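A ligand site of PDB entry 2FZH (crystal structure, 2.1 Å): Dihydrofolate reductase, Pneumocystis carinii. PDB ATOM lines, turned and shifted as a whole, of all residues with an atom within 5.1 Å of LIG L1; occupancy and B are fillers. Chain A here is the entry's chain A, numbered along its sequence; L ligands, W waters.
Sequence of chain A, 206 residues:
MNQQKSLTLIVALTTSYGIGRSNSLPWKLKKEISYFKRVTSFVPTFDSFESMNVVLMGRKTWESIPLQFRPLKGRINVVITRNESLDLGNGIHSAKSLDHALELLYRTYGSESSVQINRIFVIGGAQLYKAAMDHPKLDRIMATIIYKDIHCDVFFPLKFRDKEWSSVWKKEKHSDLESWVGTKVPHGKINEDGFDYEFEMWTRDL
Water W1 bridges the backbone carbonyl oxygen of Phe 69 and an oxygen (O4) of LIG L1.
Water W4 lies within hydrogen-bond range of an oxygen (O14) of LG2 L2 and an oxygen (O1) of LIG L1.
Water W2 lies within hydrogen-bond range of the side-chain hydroxyl (OG1) of Thr 144 (2.7 Å), the backbone carbonyl oxygen (O) of Met 142 (3.1 Å) and a nitrogen (N2) of LIG L1 (3.4 Å).
N of Ala 12 touches N2 of LIG L1 (3.5 Å).
Leu 25 touches LIG L1.
Ile 33 touches LIG L1 (CG2 to O2, 3.5 Å).
CE2 of Phe 36 touches O3 of LIG L1, at 3.4 Å.
Phe 69 touches LIG L1.
Leu 72 touches LIG L1.
Tyr 129 touches LIG L1.
Of the 20 residues printed, 14 come within 4 Å of LIG L1.
O of Ile 10 is in hydrogen-bond range of OH of Tyr 129, 2.7 Å away.
The side-chain hydroxyl (OG1) of Thr 40 is in hydrogen-bond range of the guanidinium group (NH1) of Arg 75 (3.0 Å).
O of Val 11 sits at hydrogen-bond distance from N of Thr 144, 2.8 Å away.
The backbone carbonyl oxygen of Phe 36 is in hydrogen-bond range of the side-chain hydroxyl of Thr 40 (3.0 Å).
The side-chain hydroxyl of Thr 40 is in hydrogen-bond range of the backbone carbonyl oxygen of Lys 37, at 3.4 Å.
The side-chain hydroxyl of Thr 144 lies within hydrogen-bond range of the side-chain carboxylate of Glu 32 (2.8 Å).
The side-chain hydroxyl (OH) of Tyr 129 lies within hydrogen-bond range of the backbone carbonyl oxygen (O) of Ile 123, at 3.3 Å.
N of Val 11 sits at hydrogen-bond distance from O of Met 142, at 2.8 Å.
The guanidinium group of Arg 75 is in salt-bridge range of an oxygen (O3) of LIG L1, at 2.9 Å.
The side-chain amino group (NZ) of Lys 37 lies within salt-bridge range of an oxygen (O4) of LIG L1, 3.99 Å away.
The side-chain hydroxyl of Thr 61 sits at hydrogen-bond distance from an oxygen (O2) of LG2 L2, at 3.2 Å.
The backbone carbonyl oxygen (O) of Ile 123 is in hydrogen-bond range of a nitrogen (N4) of LIG L1 (2.9 Å).
The backbone NH (N) of Val 11 sits close to a nitrogen (N3) of LIG L1, 3.4 Å away.
A nitrogen (N4) of LIG L1 is in hydrogen-bond range of the backbone carbonyl oxygen (O) of Ile 10, 3.0 Å away.
A nitrogen (N7) of LG2 L2 lies within hydrogen-bond range of the backbone carbonyl oxygen (O) of Ala 12, 2.7 Å away.
An oxygen (O14) of LG2 L2 sits at hydrogen-bond distance from the backbone NH (N) of Ala 12 (3.0 Å).
N of Thr 61 is in hydrogen-bond range of O2 of LG2 L2 (3.2 Å).
A nitrogen (N2) of LIG L1 is in hydrogen-bond range of the side-chain hydroxyl (OG1) of Thr 144, at 3.5 Å.
OE2 of Glu 32 is in hydrogen-bond range of N2 of LIG L1 (2.7 Å).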
ATOM      1  N   ILE A  10       3.342 -25.583   8.500  1.00  0.00           N
ATOM      2  CA  ILE A  10       3.221 -25.338   7.058  1.00  0.00           C
ATOM      3  C   ILE A  10       3.918 -24.016   6.726  1.00  0.00           C
ATOM      4  O   ILE A  10       3.790 -23.016   7.456  1.00  0.00           O
ATOM      5  CB  ILE A  10       1.736 -25.369   6.567  1.00  0.00           C
ATOM      6  CG1 ILE A  10       1.693 -25.158   5.040  1.00  0.00           C
ATOM      7  CG2 ILE A  10       0.897 -24.363   7.324  1.00  0.00           C
ATOM      8  CD1 ILE A  10       0.352 -25.511   4.369  1.00  0.00           C
ATOM      9  N   VAL A  11       4.674 -24.004   5.630  1.00  0.00           N
ATOM     10  CA  VAL A  11       5.435 -22.828   5.262  1.00  0.00           C
ATOM     11  C   VAL A  11       5.952 -22.890   3.832  1.00  0.00           C
ATOM     12  O   VAL A  11       6.116 -23.970   3.268  1.00  0.00           O
ATOM     13  CB  VAL A  11       6.675 -22.701   6.215  1.00  0.00           C
ATOM     14  CG1 VAL A  11       7.563 -23.959   6.069  1.00  0.00           C
ATOM     15  CG2 VAL A  11       7.480 -21.458   5.896  1.00  0.00           C
ATOM     16  N   ALA A  12       6.209 -21.707   3.266  1.00  0.00           N
ATOM     17  CA  ALA A  12       6.755 -21.562   1.931  1.00  0.00           C
ATOM     18  C   ALA A  12       8.137 -20.922   2.150  1.00  0.00           C
ATOM     19  O   ALA A  12       8.227 -19.884   2.808  1.00  0.00           O
ATOM     20  CB  ALA A  12       5.866 -20.633   1.095  1.00  0.00           C
ATOM     21  N   LEU A  25       5.455 -11.076   2.482  1.00  0.00           N
ATOM     22  CA  LEU A  25       6.072 -12.038   1.573  1.00  0.00           C
ATOM     23  C   LEU A  25       6.662 -11.359   0.358  1.00  0.00           C
ATOM     24  O   LEU A  25       5.992 -10.574  -0.316  1.00  0.00           O
ATOM     25  CB  LEU A  25       5.053 -13.081   1.124  1.00  0.00           C
ATOM     26  CG  LEU A  25       4.551 -14.070   2.170  1.00  0.00           C
ATOM     27  CD1 LEU A  25       3.555 -15.030   1.525  1.00  0.00           C
ATOM     28  CD2 LEU A  25       5.737 -14.842   2.751  1.00  0.00           C
ATOM     29  N   GLU A  32      -0.253 -20.934  -4.701  1.00  0.00           N
ATOM     30  CA  GLU A  32       0.433 -21.398  -3.489  1.00  0.00           C
ATOM     31  C   GLU A  32      -0.518 -21.218  -2.306  1.00  0.00           C
ATOM     32  O   GLU A  32      -0.762 -22.168  -1.551  1.00  0.00           O
ATOM     33  CB  GLU A  32       1.727 -20.600  -3.281  1.00  0.00           C
ATOM     34  CG  GLU A  32       2.775 -21.282  -2.396  1.00  0.00           C
ATOM     35  CD  GLU A  32       2.307 -21.490  -0.964  1.00  0.00           C
ATOM     36  OE1 GLU A  32       1.779 -20.529  -0.374  1.00  0.00           O
ATOM     37  OE2 GLU A  32       2.473 -22.599  -0.433  1.00  0.00           O
ATOM     38  N   ILE A  33      -1.092 -20.016  -2.165  1.00  0.00           N
ATOM     39  CA  ILE A  33      -2.045 -19.746  -1.084  1.00  0.00           C
ATOM     40  C   ILE A  33      -3.252 -20.676  -1.170  1.00  0.00           C
ATOM     41  O   ILE A  33      -3.801 -21.075  -0.142  1.00  0.00           O
ATOM     42  CB  ILE A  33      -2.552 -18.274  -1.112  1.00  0.00           C
ATOM     43  CG1 ILE A  33      -1.361 -17.318  -1.055  1.00  0.00           C
ATOM     44  CG2 ILE A  33      -3.433 -18.006   0.093  1.00  0.00           C
ATOM     45  CD1 ILE A  33      -0.475 -17.528   0.139  1.00  0.00           C
ATOM     46  N   TYR A  35      -3.236 -23.681  -2.095  1.00  0.00           N
ATOM     47  CA  TYR A  35      -2.765 -24.928  -1.527  1.00  0.00           C
ATOM     48  C   TYR A  35      -2.813 -24.821  -0.008  1.00  0.00           C
ATOM     49  O   TYR A  35      -3.290 -25.728   0.675  1.00  0.00           O
ATOM     50  CB  TYR A  35      -1.324 -25.158  -1.940  1.00  0.00           C
ATOM     51  CG  TYR A  35      -0.672 -26.307  -1.233  1.00  0.00           C
ATOM     52  CD1 TYR A  35      -0.922 -27.625  -1.618  1.00  0.00           C
ATOM     53  CD2 TYR A  35       0.250 -26.089  -0.220  1.00  0.00           C
ATOM     54  CE1 TYR A  35      -0.278 -28.686  -1.021  1.00  0.00           C
ATOM     55  CE2 TYR A  35       0.905 -27.158   0.394  1.00  0.00           C
ATOM     56  CZ  TYR A  35       0.649 -28.439  -0.015  1.00  0.00           C
ATOM     57  OH  TYR A  35       1.333 -29.485   0.542  1.00  0.00           O
ATOM     58  N   PHE A  36      -2.309 -23.703   0.510  1.00  0.00           N
ATOM     59  CA  PHE A  36      -2.290 -23.469   1.954  1.00  0.00           C
ATOM     60  C   PHE A  36      -3.689 -23.694   2.505  1.00  0.00           C
ATOM     61  O   PHE A  36      -3.878 -24.471   3.443  1.00  0.00           O
ATOM     62  CB  PHE A  36      -1.846 -22.032   2.282  1.00  0.00           C
ATOM     63  CG  PHE A  36      -2.133 -21.617   3.698  1.00  0.00           C
ATOM     64  CD1 PHE A  36      -1.317 -22.041   4.741  1.00  0.00           C
ATOM     65  CD2 PHE A  36      -3.263 -20.875   3.993  1.00  0.00           C
ATOM     66  CE1 PHE A  36      -1.631 -21.724   6.080  1.00  0.00           C
ATOM     67  CE2 PHE A  36      -3.595 -20.550   5.307  1.00  0.00           C
ATOM     68  CZ  PHE A  36      -2.772 -20.975   6.358  1.00  0.00           C
ATOM     69  N   LYS A  37      -4.658 -23.003   1.917  1.00  0.00           N
ATOM     70  CA  LYS A  37      -6.056 -23.084   2.329  1.00  0.00           C
ATOM     71  C   LYS A  37      -6.569 -24.531   2.332  1.00  0.00           C
ATOM     72  O   LYS A  37      -7.100 -24.999   3.348  1.00  0.00           O
ATOM     73  CB  LYS A  37      -6.933 -22.246   1.392  1.00  0.00           C
ATOM     74  CG  LYS A  37      -8.401 -22.241   1.767  1.00  0.00           C
ATOM     75  CD  LYS A  37      -9.229 -21.248   0.937  1.00  0.00           C
ATOM     76  CE  LYS A  37     -10.638 -21.120   1.508  1.00  0.00           C
ATOM     77  NZ  LYS A  37     -11.338 -19.886   1.020  1.00  0.00           N
ATOM     78  N   THR A  40      -4.792 -26.679   5.179  1.00  0.00           N
ATOM     79  CA  THR A  40      -5.217 -26.378   6.542  1.00  0.00           C
ATOM     80  C   THR A  40      -6.704 -26.519   6.822  1.00  0.00           C
ATOM     81  O   THR A  40      -7.105 -26.630   7.976  1.00  0.00           O
ATOM     82  CB  THR A  40      -4.776 -24.967   6.971  1.00  0.00           C
ATOM     83  OG1 THR A  40      -5.297 -24.014   6.031  1.00  0.00           O
ATOM     84  CG2 THR A  40      -3.243 -24.883   6.997  1.00  0.00           C
ATOM     85  N   THR A  61       1.916 -12.260  12.104  1.00  0.00           N
ATOM     86  CA  THR A  61       1.361 -12.890  10.914  1.00  0.00           C
ATOM     87  C   THR A  61      -0.135 -12.579  10.862  1.00  0.00           C
ATOM     88  O   THR A  61      -0.682 -12.267   9.806  1.00  0.00           O
ATOM     89  CB  THR A  61       1.609 -14.417  10.917  1.00  0.00           C
ATOM     90  OG1 THR A  61       3.015 -14.650  10.759  1.00  0.00           O
ATOM     91  CG2 THR A  61       0.870 -15.106   9.783  1.00  0.00           C
ATOM     92  N   ILE A  65      -2.064 -10.458   7.553  1.00  0.00           N
ATOM     93  CA  ILE A  65      -3.058 -11.077   6.683  1.00  0.00           C
ATOM     94  C   ILE A  65      -4.226 -10.128   6.444  1.00  0.00           C
ATOM     95  O   ILE A  65      -4.739  -9.491   7.378  1.00  0.00           O
ATOM     96  CB  ILE A  65      -3.589 -12.385   7.314  1.00  0.00           C
ATOM     97  CG1 ILE A  65      -2.430 -13.360   7.523  1.00  0.00           C
ATOM     98  CG2 ILE A  65      -4.671 -12.985   6.417  1.00  0.00           C
ATOM     99  CD1 ILE A  65      -2.811 -14.650   8.202  1.00  0.00           C
ATOM    100  N   PHE A  69      -9.704 -11.833   4.461  1.00  0.00           N
ATOM    101  CA  PHE A  69      -9.416 -13.261   4.555  1.00  0.00           C
ATOM    102  C   PHE A  69      -9.239 -13.689   6.015  1.00  0.00           C
ATOM    103  O   PHE A  69      -8.896 -14.850   6.297  1.00  0.00           O
ATOM    104  CB  PHE A  69      -8.157 -13.587   3.755  1.00  0.00           C
ATOM    105  CG  PHE A  69      -8.198 -13.111   2.329  1.00  0.00           C
ATOM    106  CD1 PHE A  69      -9.169 -13.590   1.454  1.00  0.00           C
ATOM    107  CD2 PHE A  69      -7.291 -12.172   1.869  1.00  0.00           C
ATOM    108  CE1 PHE A  69      -9.225 -13.125   0.139  1.00  0.00           C
ATOM    109  CE2 PHE A  69      -7.339 -11.697   0.560  1.00  0.00           C
ATOM    110  CZ  PHE A  69      -8.316 -12.173  -0.309  1.00  0.00           C
ATOM    111  N   LEU A  72      -9.254 -16.964   9.337  1.00  0.00           N
ATOM    112  CA  LEU A  72      -9.246 -18.072   8.384  1.00  0.00           C
ATOM    113  C   LEU A  72     -10.523 -18.857   8.574  1.00  0.00           C
ATOM    114  O   LEU A  72     -10.738 -19.491   9.607  1.00  0.00           O
ATOM    115  CB  LEU A  72      -8.043 -18.987   8.615  1.00  0.00           C
ATOM    116  CG  LEU A  72      -6.678 -18.316   8.571  1.00  0.00           C
ATOM    117  CD1 LEU A  72      -5.571 -19.366   8.449  1.00  0.00           C
ATOM    118  CD2 LEU A  72      -6.620 -17.365   7.398  1.00  0.00           C
ATOM    119  N   ARG A  75     -11.817 -22.862   9.841  1.00  0.00           N
ATOM    120  CA  ARG A  75     -10.787 -23.336  10.753  1.00  0.00           C
ATOM    121  C   ARG A  75     -10.787 -22.546  12.071  1.00  0.00           C
ATOM    122  O   ARG A  75     -11.173 -21.368  12.119  1.00  0.00           O
ATOM    123  CB  ARG A  75      -9.389 -23.203  10.088  1.00  0.00           C
ATOM    124  CG  ARG A  75      -9.141 -24.139   8.905  1.00  0.00           C
ATOM    125  CD  ARG A  75      -8.282 -23.483   7.823  1.00  0.00           C
ATOM    126  NE  ARG A  75      -8.926 -22.269   7.297  1.00  0.00           N
ATOM    127  CZ  ARG A  75      -8.419 -21.474   6.358  1.00  0.00           C
ATOM    128  NH1 ARG A  75      -7.243 -21.742   5.813  1.00  0.00           N
ATOM    129  NH2 ARG A  75      -9.092 -20.398   5.969  1.00  0.00           N
ATOM    130  N   ILE A 123       1.192 -21.931  11.352  1.00  0.00           N
ATOM    131  CA  ILE A 123       1.298 -21.249  10.058  1.00  0.00           C
ATOM    132  C   ILE A 123       1.936 -19.877  10.054  1.00  0.00           C
ATOM    133  O   ILE A 123       2.296 -19.370   8.989  1.00  0.00           O
ATOM    134  CB  ILE A 123      -0.106 -21.044   9.442  1.00  0.00           C
ATOM    135  CG1 ILE A 123      -0.836 -19.905  10.181  1.00  0.00           C
ATOM    136  CG2 ILE A 123      -0.920 -22.310   9.577  1.00  0.00           C
ATOM    137  CD1 ILE A 123      -2.281 -19.679   9.698  1.00  0.00           C
ATOM    138  N   GLY A 124       2.072 -19.275  11.216  1.00  0.00           N
ATOM    139  CA  GLY A 124       2.592 -17.922  11.216  1.00  0.00           C
ATOM    140  C   GLY A 124       3.732 -17.502  12.101  1.00  0.00           C
ATOM    141  O   GLY A 124       3.786 -17.843  13.282  1.00  0.00           O
ATOM    142  N   TYR A 129       7.619 -20.138  14.513  1.00  0.00           N
ATOM    143  CA  TYR A 129       8.266 -21.271  13.866  1.00  0.00           C
ATOM    144  C   TYR A 129       9.378 -21.771  14.772  1.00  0.00           C
ATOM    145  O   TYR A 129       9.554 -22.986  14.928  1.00  0.00           O
ATOM    146  CB  TYR A 129       8.855 -20.866  12.510  1.00  0.00           C
ATOM    147  CG  TYR A 129       7.854 -20.820  11.370  1.00  0.00           C
ATOM    148  CD1 TYR A 129       6.682 -21.580  11.402  1.00  0.00           C
ATOM    149  CD2 TYR A 129       8.088 -20.048  10.236  1.00  0.00           C
ATOM    150  CE1 TYR A 129       5.780 -21.564  10.337  1.00  0.00           C
ATOM    151  CE2 TYR A 129       7.209 -20.027   9.163  1.00  0.00           C
ATOM    152  CZ  TYR A 129       6.041 -20.799   9.235  1.00  0.00           C
ATOM    153  OH  TYR A 129       5.152 -20.781   8.184  1.00  0.00           O
ATOM    154  N   MET A 142       4.915 -29.157   6.097  1.00  0.00           N
ATOM    155  CA  MET A 142       4.324 -28.991   4.764  1.00  0.00           C
ATOM    156  C   MET A 142       5.135 -27.815   4.265  1.00  0.00           C
ATOM    157  O   MET A 142       4.913 -26.660   4.670  1.00  0.00           O
ATOM    158  CB  MET A 142       2.845 -28.616   4.855  1.00  0.00           C
ATOM    159  CG  MET A 142       1.931 -29.658   5.524  1.00  0.00           C
ATOM    160  SD  MET A 142       2.325 -31.371   5.057  1.00  0.00           S
ATOM    161  CE  MET A 142       1.570 -31.496   3.489  1.00  0.00           C
ATOM    162  N   THR A 144       6.763 -25.544   1.026  1.00  0.00           N
ATOM    163  CA  THR A 144       6.689 -25.215  -0.385  1.00  0.00           C
ATOM    164  C   THR A 144       8.067 -24.600  -0.685  1.00  0.00           C
ATOM    165  O   THR A 144       8.360 -23.488  -0.255  1.00  0.00           O
ATOM    166  CB  THR A 144       5.575 -24.179  -0.697  1.00  0.00           C
ATOM    167  OG1 THR A 144       4.294 -24.717  -0.358  1.00  0.00           O
ATOM    168  CG2 THR A 144       5.603 -23.823  -2.180  1.00  0.00           C
HETATM  169  C1  LIG L   1       2.354 -15.072   5.278  1.00  0.00           C
HETATM  170  O1  LIG L   1       1.967 -16.153   4.409  1.00  0.00           O
HETATM  171  C2  LIG L   1       0.590 -16.242   4.137  1.00  0.00           C
HETATM  172  C3  LIG L   1      -0.066 -15.210   3.416  1.00  0.00           C
HETATM  173  C4  LIG L   1      -1.464 -15.260   3.120  1.00  0.00           C
HETATM  174  C5  LIG L   1      -2.184 -16.374   3.554  1.00  0.00           C
HETATM  175  O2  LIG L   1      -3.552 -16.419   3.257  1.00  0.00           O
HETATM  176  C6  LIG L   1      -4.437 -16.695   4.374  1.00  0.00           C
HETATM  177  C7  LIG L   1      -5.897 -16.307   3.989  1.00  0.00           C
HETATM  178  C8  LIG L   1      -6.311 -16.646   2.516  1.00  0.00           C
HETATM  179  C9  LIG L   1      -6.317 -18.135   2.162  1.00  0.00           C
HETATM  180  C10 LIG L   1      -7.081 -18.983   3.170  1.00  0.00           C
HETATM  181  O3  LIG L   1      -6.508 -19.844   3.803  1.00  0.00           O
HETATM  182  O4  LIG L   1      -8.279 -18.793   3.341  1.00  0.00           O
HETATM  183  C11 LIG L   1      -1.543 -17.451   4.293  1.00  0.00           C
HETATM  184  C12 LIG L   1      -0.148 -17.383   4.577  1.00  0.00           C
HETATM  185  C13 LIG L   1       0.590 -18.509   5.352  1.00  0.00           C
HETATM  186  C14 LIG L   1       1.215 -19.633   4.477  1.00  0.00           C
HETATM  187  C15 LIG L   1       1.130 -19.692   3.054  1.00  0.00           C
HETATM  188  N1  LIG L   1       1.725 -20.725   2.352  1.00  0.00           N
HETATM  189  C16 LIG L   1       2.392 -21.720   2.976  1.00  0.00           C
HETATM  190  N2  LIG L   1       2.995 -22.766   2.226  1.00  0.00           N
HETATM  191  N3  LIG L   1       2.507 -21.727   4.321  1.00  0.00           N
HETATM  192  C17 LIG L   1       1.921 -20.695   5.111  1.00  0.00           C
HETATM  193  N4  LIG L   1       2.054 -20.736   6.414  1.00  0.00           N
HETATM  194  P1  LG2 L   2       5.362 -13.856  14.226  1.00  0.00           P
HETATM  195  O1  LG2 L   2       5.845 -14.943  14.813  1.00  0.00           O
HETATM  196  O2  LG2 L   2       4.121 -13.962  13.647  1.00  0.00           O
HETATM  197  O3  LG2 L   2       5.398 -12.541  15.120  1.00  0.00           O
HETATM  198  C1  LG2 L   2       5.999 -12.632  16.507  1.00  0.00           C
HETATM  199  C2  LG2 L   2       5.133 -12.013  17.543  1.00  0.00           C
HETATM  200  O4  LG2 L   2       4.158 -13.050  17.772  1.00  0.00           O
HETATM  201  C3  LG2 L   2       5.718 -11.896  18.914  1.00  0.00           C
HETATM  202  O5  LG2 L   2       6.038 -10.579  18.928  1.00  0.00           O
HETATM  203  C4  LG2 L   2       4.590 -12.296  19.913  1.00  0.00           C
HETATM  204  O6  LG2 L   2       3.554 -11.378  20.186  1.00  0.00           O
HETATM  205  C5  LG2 L   2       4.145 -13.575  19.130  1.00  0.00           C
HETATM  206  N1  LG2 L   2       4.866 -14.855  19.367  1.00  0.00           N
HETATM  207  C6  LG2 L   2       5.564 -15.625  18.447  1.00  0.00           C
HETATM  208  N2  LG2 L   2       6.114 -16.695  18.899  1.00  0.00           N
HETATM  209  C7  LG2 L   2       5.724 -16.621  20.261  1.00  0.00           C
HETATM  210  C8  LG2 L   2       5.937 -17.422  21.385  1.00  0.00           C
HETATM  211  N3  LG2 L   2       6.666 -18.564  21.216  1.00  0.00           N
HETATM  212  N4  LG2 L   2       5.432 -17.102  22.684  1.00  0.00           N
HETATM  213  C9  LG2 L   2       4.674 -15.921  22.865  1.00  0.00           C
HETATM  214  N5  LG2 L   2       4.443 -15.095  21.742  1.00  0.00           N
HETATM  215  C10 LG2 L   2       4.990 -15.490  20.506  1.00  0.00           C
HETATM  216  O7  LG2 L   2       6.181 -13.338  13.069  1.00  0.00           O
HETATM  217  P2  LG2 L   2       7.681 -12.943  12.769  1.00  0.00           P
HETATM  218  O8  LG2 L   2       7.815 -11.646  13.113  1.00  0.00           O
HETATM  219  O9  LG2 L   2       8.504 -13.776  13.522  1.00  0.00           O
HETATM  220  O10 LG2 L   2       7.850 -13.068  11.219  1.00  0.00           O
HETATM  221  C11 LG2 L   2       7.205 -12.396  10.407  1.00  0.00           C
HETATM  222  C12 LG2 L   2       7.680 -12.795   9.019  1.00  0.00           C
HETATM  223  O11 LG2 L   2       7.353 -14.286   8.764  1.00  0.00           O
HETATM  224  C13 LG2 L   2       7.009 -12.026   7.781  1.00  0.00           C
HETATM  225  O12 LG2 L   2       7.767 -11.674   6.585  1.00  0.00           O
HETATM  226  C14 LG2 L   2       5.821 -12.939   7.523  1.00  0.00           C
HETATM  227  O13 LG2 L   2       5.156 -12.842   6.280  1.00  0.00           O
HETATM  228  C15 LG2 L   2       6.623 -14.248   7.491  1.00  0.00           C
HETATM  229  N6  LG2 L   2       5.809 -15.504   7.252  1.00  0.00           N
HETATM  230  C16 LG2 L   2       6.206 -16.313   6.097  1.00  0.00           C
HETATM  231  C17 LG2 L   2       5.500 -17.477   5.843  1.00  0.00           C
HETATM  232  C18 LG2 L   2       5.918 -18.242   4.707  1.00  0.00           C
HETATM  233  O14 LG2 L   2       5.223 -19.247   4.595  1.00  0.00           O
HETATM  234  N7  LG2 L   2       6.956 -17.827   3.958  1.00  0.00           N
HETATM  235  C19 LG2 L   2       4.370 -17.769   6.808  1.00  0.00           C
HETATM  236  C20 LG2 L   2       3.974 -16.951   7.960  1.00  0.00           C
HETATM  237  C21 LG2 L   2       4.727 -15.820   8.158  1.00  0.00           C
HETATM  238  P3  LG2 L   2       3.479 -10.051  20.922  1.00  0.00           P
HETATM  239  O15 LG2 L   2       4.550  -9.239  20.358  1.00  0.00           O
HETATM  240  O16 LG2 L   2       2.091  -9.678  20.775  1.00  0.00           O
HETATM  241  O17 LG2 L   2       3.774 -10.657  22.297  1.00  0.00           O
HETATM  242  O   HOH W   1      -9.776 -17.044   4.982  1.00  0.00           O
HETATM  243  O   HOH W   2       3.691 -26.120   1.886  1.00  0.00           O
HETATM  244  O   HOH W   3       2.838 -11.972   5.842  1.00  0.00           O
HETATM  245  O   HOH W   4       3.580 -18.075   2.492  1.00  0.00           O
